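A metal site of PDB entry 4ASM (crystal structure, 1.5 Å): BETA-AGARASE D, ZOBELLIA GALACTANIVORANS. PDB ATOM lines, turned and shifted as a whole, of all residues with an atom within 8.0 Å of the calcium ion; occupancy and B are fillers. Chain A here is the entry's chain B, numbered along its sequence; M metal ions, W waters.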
ATOM      1  N   TYR A   8     -19.346  30.312 -21.889  1.00  0.00           N
ATOM      2  CA  TYR A   8     -18.720  28.998 -22.041  1.00  0.00           C
ATOM      3  C   TYR A   8     -18.274  28.494 -20.688  1.00  0.00           C
ATOM      4  O   TYR A   8     -17.999  29.302 -19.783  1.00  0.00           O
ATOM      5  CB  TYR A   8     -17.485  29.081 -22.916  1.00  0.00           C
ATOM      6  CG  TYR A   8     -17.719  29.631 -24.307  1.00  0.00           C
ATOM      7  CD1 TYR A   8     -18.238  28.832 -25.302  1.00  0.00           C
ATOM      8  CD2 TYR A   8     -17.391  30.947 -24.605  1.00  0.00           C
ATOM      9  CE1 TYR A   8     -18.437  29.331 -26.578  1.00  0.00           C
ATOM     10  CE2 TYR A   8     -17.592  31.463 -25.878  1.00  0.00           C
ATOM     11  CZ  TYR A   8     -18.109  30.636 -26.857  1.00  0.00           C
ATOM     12  OH  TYR A   8     -18.328  31.137 -28.123  1.00  0.00           O
ATOM     13  N   ASP A   9     -18.169  27.161 -20.559  1.00  0.00           N
ATOM     14  CA  ASP A   9     -17.752  26.543 -19.300  1.00  0.00           C
ATOM     15  C   ASP A   9     -16.425  27.068 -18.769  1.00  0.00           C
ATOM     16  O   ASP A   9     -16.199  27.055 -17.551  1.00  0.00           O
ATOM     17  CB  ASP A   9     -17.609  25.026 -19.469  1.00  0.00           C
ATOM     18  CG  ASP A   9     -18.949  24.314 -19.573  1.00  0.00           C
ATOM     19  OD1 ASP A   9     -20.002  24.910 -19.264  1.00  0.00           O
ATOM     20  OD2 ASP A   9     -18.947  23.118 -19.947  1.00  0.00           O
ATOM     21  N   TRP A  10     -15.547  27.490 -19.675  1.00  0.00           N
ATOM     22  CA  TRP A  10     -14.190  27.902 -19.344  1.00  0.00           C
ATOM     23  C   TRP A  10     -14.084  29.398 -19.103  1.00  0.00           C
ATOM     24  O   TRP A  10     -12.984  29.924 -18.942  1.00  0.00           O
ATOM     25  CB  TRP A  10     -13.201  27.521 -20.464  1.00  0.00           C
ATOM     26  CG  TRP A  10     -13.613  28.037 -21.822  1.00  0.00           C
ATOM     27  CD1 TRP A  10     -13.547  29.330 -22.267  1.00  0.00           C
ATOM     28  CD2 TRP A  10     -14.180  27.265 -22.887  1.00  0.00           C
ATOM     29  NE1 TRP A  10     -14.016  29.407 -23.560  1.00  0.00           N
ATOM     30  CE2 TRP A  10     -14.430  28.159 -23.957  1.00  0.00           C
ATOM     31  CE3 TRP A  10     -14.482  25.895 -23.052  1.00  0.00           C
ATOM     32  CZ2 TRP A  10     -14.957  27.731 -25.181  1.00  0.00           C
ATOM     33  CZ3 TRP A  10     -15.028  25.488 -24.274  1.00  0.00           C
ATOM     34  CH2 TRP A  10     -15.271  26.405 -25.307  1.00  0.00           C
ATOM     35  N   ASP A  33     -15.319  23.533 -27.894  1.00  0.00           N
ATOM     36  CA  ASP A  33     -16.558  22.858 -27.571  1.00  0.00           C
ATOM     37  C   ASP A  33     -16.656  22.623 -26.063  1.00  0.00           C
ATOM     38  O   ASP A  33     -15.768  21.974 -25.476  1.00  0.00           O
ATOM     39  CB  ASP A  33     -16.636  21.509 -28.322  1.00  0.00           C
ATOM     40  CG  ASP A  33     -18.045  20.963 -28.400  1.00  0.00           C
ATOM     41  OD1 ASP A  33     -18.914  21.448 -27.629  1.00  0.00           O
ATOM     42  OD2 ASP A  33     -18.267  20.046 -29.216  1.00  0.00           O
ATOM     43  N   ASP A  34     -17.710  23.133 -25.425  1.00  0.00           N
ATOM     44  CA  ASP A  34     -17.934  22.774 -24.021  1.00  0.00           C
ATOM     45  C   ASP A  34     -18.963  21.668 -23.789  1.00  0.00           C
ATOM     46  O   ASP A  34     -19.367  21.420 -22.629  1.00  0.00           O
ATOM     47  CB  ASP A  34     -18.127  24.009 -23.091  1.00  0.00           C
ATOM     48  CG  ASP A  34     -19.314  24.882 -23.458  1.00  0.00           C
ATOM     49  OD1 ASP A  34     -20.024  24.563 -24.442  1.00  0.00           O
ATOM     50  OD2 ASP A  34     -19.500  25.909 -22.742  1.00  0.00           O
ATOM     51  N   PHE A  35     -19.361  20.979 -24.863  1.00  0.00           N
ATOM     52  CA  PHE A  35     -20.065  19.686 -24.792  1.00  0.00           C
ATOM     53  C   PHE A  35     -21.323  19.668 -23.928  1.00  0.00           C
ATOM     54  O   PHE A  35     -21.564  18.714 -23.199  1.00  0.00           O
ATOM     55  CB  PHE A  35     -19.108  18.586 -24.280  1.00  0.00           C
ATOM     56  CG  PHE A  35     -17.932  18.319 -25.196  1.00  0.00           C
ATOM     57  CD1 PHE A  35     -18.154  17.861 -26.493  1.00  0.00           C
ATOM     58  CD2 PHE A  35     -16.608  18.471 -24.758  1.00  0.00           C
ATOM     59  CE1 PHE A  35     -17.093  17.585 -27.348  1.00  0.00           C
ATOM     60  CE2 PHE A  35     -15.538  18.184 -25.613  1.00  0.00           C
ATOM     61  CZ  PHE A  35     -15.777  17.757 -26.899  1.00  0.00           C
ATOM     62  N   ASN A  36     -22.164  20.698 -24.060  1.00  0.00           N
ATOM     63  CA  ASN A  36     -23.332  20.804 -23.167  1.00  0.00           C
ATOM     64  C   ASN A  36     -24.662  20.415 -23.830  1.00  0.00           C
ATOM     65  O   ASN A  36     -25.742  20.463 -23.216  1.00  0.00           O
ATOM     66  CB  ASN A  36     -23.347  22.170 -22.493  1.00  0.00           C
ATOM     67  CG  ASN A  36     -22.180  22.334 -21.528  1.00  0.00           C
ATOM     68  OD1 ASN A  36     -21.643  21.336 -21.009  1.00  0.00           O
ATOM     69  ND2 ASN A  36     -21.748  23.571 -21.308  1.00  0.00           N
ATOM     70  N   TYR A  37     -24.541  19.923 -25.052  1.00  0.00           N
ATOM     71  CA  TYR A  37     -25.643  19.498 -25.882  1.00  0.00           C
ATOM     72  C   TYR A  37     -25.804  17.984 -25.804  1.00  0.00           C
ATOM     73  O   TYR A  37     -25.053  17.302 -25.092  1.00  0.00           O
ATOM     74  CB  TYR A  37     -25.380  19.958 -27.319  1.00  0.00           C
ATOM     75  CG  TYR A  37     -24.032  19.540 -27.891  1.00  0.00           C
ATOM     76  CD1 TYR A  37     -22.884  20.303 -27.668  1.00  0.00           C
ATOM     77  CD2 TYR A  37     -23.918  18.368 -28.636  1.00  0.00           C
ATOM     78  CE1 TYR A  37     -21.646  19.908 -28.191  1.00  0.00           C
ATOM     79  CE2 TYR A  37     -22.687  17.958 -29.143  1.00  0.00           C
ATOM     80  CZ  TYR A  37     -21.573  18.746 -28.921  1.00  0.00           C
ATOM     81  OH  TYR A  37     -20.360  18.330 -29.441  1.00  0.00           O
ATOM     82  N   VAL A  86     -22.363  12.685 -26.483  1.00  0.00           N
ATOM     83  CA  VAL A  86     -22.258  13.914 -25.690  1.00  0.00           C
ATOM     84  C   VAL A  86     -23.535  13.975 -24.870  1.00  0.00           C
ATOM     85  O   VAL A  86     -24.627  13.873 -25.430  1.00  0.00           O
ATOM     86  CB  VAL A  86     -22.062  15.175 -26.561  1.00  0.00           C
ATOM     87  CG1 VAL A  86     -21.872  16.437 -25.710  1.00  0.00           C
ATOM     88  CG2 VAL A  86     -20.855  14.973 -27.483  1.00  0.00           C
ATOM     89  N   SER A  87     -23.382  14.110 -23.549  1.00  0.00           N
ATOM     90  CA  SER A  87     -24.531  14.184 -22.638  1.00  0.00           C
ATOM     91  C   SER A  87     -24.068  14.537 -21.246  1.00  0.00           C
ATOM     92  O   SER A  87     -22.923  14.264 -20.873  1.00  0.00           O
ATOM     93  CB  SER A  87     -25.350  12.887 -22.609  1.00  0.00           C
ATOM     94  OG  SER A  87     -24.549  11.805 -22.157  1.00  0.00           O
ATOM     95  N   GLY A  88     -24.946  15.193 -20.472  1.00  0.00           N
ATOM     96  CA  GLY A  88     -24.641  15.483 -19.071  1.00  0.00           C
ATOM     97  C   GLY A  88     -23.543  16.514 -18.904  1.00  0.00           C
ATOM     98  O   GLY A  88     -22.946  16.645 -17.836  1.00  0.00           O
ATOM     99  N   GLY A  89     -23.282  17.262 -19.978  1.00  0.00           N
ATOM    100  CA  GLY A  89     -22.251  18.290 -19.968  1.00  0.00           C
ATOM    101  C   GLY A  89     -20.871  17.818 -20.413  1.00  0.00           C
ATOM    102  O   GLY A  89     -19.926  18.595 -20.418  1.00  0.00           O
ATOM    103  N   ASN A  90     -20.757  16.560 -20.799  1.00  0.00           N
ATOM    104  CA  ASN A  90     -19.454  15.988 -21.159  1.00  0.00           C
ATOM    105  C   ASN A  90     -19.501  15.261 -22.493  1.00  0.00           C
ATOM    106  O   ASN A  90     -20.503  14.604 -22.814  1.00  0.00           O
ATOM    107  CB  ASN A  90     -19.002  14.944 -20.134  1.00  0.00           C
ATOM    108  CG  ASN A  90     -18.833  15.490 -18.729  1.00  0.00           C
ATOM    109  OD1 ASN A  90     -17.975  16.336 -18.475  1.00  0.00           O
ATOM    110  ND2 ASN A  90     -19.644  14.976 -17.801  1.00  0.00           N
ATOM    111  N   LEU A  91     -18.383  15.310 -23.223  1.00  0.00           N
ATOM    112  CA  LEU A  91     -18.101  14.267 -24.190  1.00  0.00           C
ATOM    113  C   LEU A  91     -17.846  12.963 -23.415  1.00  0.00           C
ATOM    114  O   LEU A  91     -17.084  12.961 -22.433  1.00  0.00           O
ATOM    115  CB  LEU A  91     -16.857  14.646 -24.996  1.00  0.00           C
ATOM    116  CG  LEU A  91     -16.253  13.600 -25.936  1.00  0.00           C
ATOM    117  CD1 LEU A  91     -17.163  13.299 -27.161  1.00  0.00           C
ATOM    118  CD2 LEU A  91     -14.846  14.015 -26.361  1.00  0.00           C
ATOM    119  N   ARG A 138     -10.603  20.108 -20.138  1.00  0.00           N
ATOM    120  CA  ARG A 138     -10.901  19.679 -18.776  1.00  0.00           C
ATOM    121  C   ARG A 138     -11.481  18.281 -18.912  1.00  0.00           C
ATOM    122  O   ARG A 138     -12.484  18.064 -19.578  1.00  0.00           O
ATOM    123  CB  ARG A 138     -11.873  20.613 -18.072  1.00  0.00           C
ATOM    124  CG  ARG A 138     -12.139  20.207 -16.638  1.00  0.00           C
ATOM    125  CD  ARG A 138     -12.910  21.324 -15.896  1.00  0.00           C
ATOM    126  NE  ARG A 138     -13.032  20.977 -14.466  1.00  0.00           N
ATOM    127  CZ  ARG A 138     -14.075  20.349 -13.924  1.00  0.00           C
ATOM    128  NH1 ARG A 138     -15.112  19.985 -14.671  1.00  0.00           N
ATOM    129  NH2 ARG A 138     -14.059  20.055 -12.629  1.00  0.00           N
ATOM    130  N   VAL A 353     -14.924  14.344 -21.076  1.00  0.00           N
ATOM    131  CA  VAL A 353     -14.322  15.643 -21.339  1.00  0.00           C
ATOM    132  C   VAL A 353     -15.401  16.721 -21.176  1.00  0.00           C
ATOM    133  O   VAL A 353     -16.378  16.804 -21.917  1.00  0.00           O
ATOM    134  CB  VAL A 353     -13.657  15.737 -22.734  1.00  0.00           C
ATOM    135  CG1 VAL A 353     -13.000  17.099 -22.925  1.00  0.00           C
ATOM    136  CG2 VAL A 353     -12.631  14.587 -22.950  1.00  0.00           C
ATOM    137  N   ASP A 354     -15.207  17.546 -20.150  1.00  0.00           N
ATOM    138  CA  ASP A 354     -16.140  18.632 -19.863  1.00  0.00           C
ATOM    139  C   ASP A 354     -16.092  19.692 -20.959  1.00  0.00           C
ATOM    140  O   ASP A 354     -17.132  20.209 -21.382  1.00  0.00           O
ATOM    141  CB  ASP A 354     -15.757  19.207 -18.500  1.00  0.00           C
ATOM    142  CG  ASP A 354     -16.711  20.281 -17.981  1.00  0.00           C
ATOM    143  OD1 ASP A 354     -17.837  20.458 -18.531  1.00  0.00           O
ATOM    144  OD2 ASP A 354     -16.329  20.943 -17.007  1.00  0.00           O
ATOM    145  N   TRP A 355     -14.882  20.011 -21.407  1.00  0.00           N
ATOM    146  CA  TRP A 355     -14.703  21.005 -22.453  1.00  0.00           C
ATOM    147  C   TRP A 355     -13.306  20.931 -23.048  1.00  0.00           C
ATOM    148  O   TRP A 355     -12.380  20.426 -22.416  1.00  0.00           O
ATOM    149  CB  TRP A 355     -14.971  22.421 -21.927  1.00  0.00           C
ATOM    150  CG  TRP A 355     -14.269  22.887 -20.670  1.00  0.00           C
ATOM    151  CD1 TRP A 355     -14.859  23.017 -19.441  1.00  0.00           C
ATOM    152  CD2 TRP A 355     -12.924  23.393 -20.527  1.00  0.00           C
ATOM    153  NE1 TRP A 355     -13.954  23.538 -18.535  1.00  0.00           N
ATOM    154  CE2 TRP A 355     -12.769  23.771 -19.174  1.00  0.00           C
ATOM    155  CE3 TRP A 355     -11.816  23.525 -21.395  1.00  0.00           C
ATOM    156  CZ2 TRP A 355     -11.567  24.291 -18.664  1.00  0.00           C
ATOM    157  CZ3 TRP A 355     -10.622  24.039 -20.888  1.00  0.00           C
ATOM    158  CH2 TRP A 355     -10.512  24.433 -19.527  1.00  0.00           C
ATOM    159  N   ILE A 356     -13.188  21.421 -24.271  1.00  0.00           N
ATOM    160  CA  ILE A 356     -11.911  21.631 -24.918  1.00  0.00           C
ATOM    161  C   ILE A 356     -11.958  22.999 -25.600  1.00  0.00           C
ATOM    162  O   ILE A 356     -12.901  23.317 -26.335  1.00  0.00           O
ATOM    163  CB  ILE A 356     -11.558  20.474 -25.890  1.00  0.00           C
ATOM    164  CG1 ILE A 356     -10.134  20.628 -26.451  1.00  0.00           C
ATOM    165  CG2 ILE A 356     -12.630  20.315 -26.989  1.00  0.00           C
ATOM    166  CD1 ILE A 356      -9.662  19.392 -27.193  1.00  0.00           C
HETATM  167 CA    CA M   1     -19.292  20.869 -20.334  1.00  0.00          CA
HETATM  168  O   HOH W   1     -20.651  20.839 -18.325  1.00  0.00           O
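The guanidinium group (NH1) of Arg 138 is in salt-bridge range of the side-chain carboxylate (OD2) of Asp 354 (2.8 Å).
The backbone NH (N) of Asp 354 sits close to the side-chain amide oxygen (OD1) of Asn 90, 3.5 Å away.
The calcium ion is bound by OD2 of Asp 9 (2.3 Å), OD1 of Asp 354 (2.4 Å), O of Asp 34 (2.4 Å), O of Gly 89 (2.4 Å), water W1 (2.4 Å), O of Asp 354 (2.5 Å) and OD1 of Asn 36 (2.5 Å).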
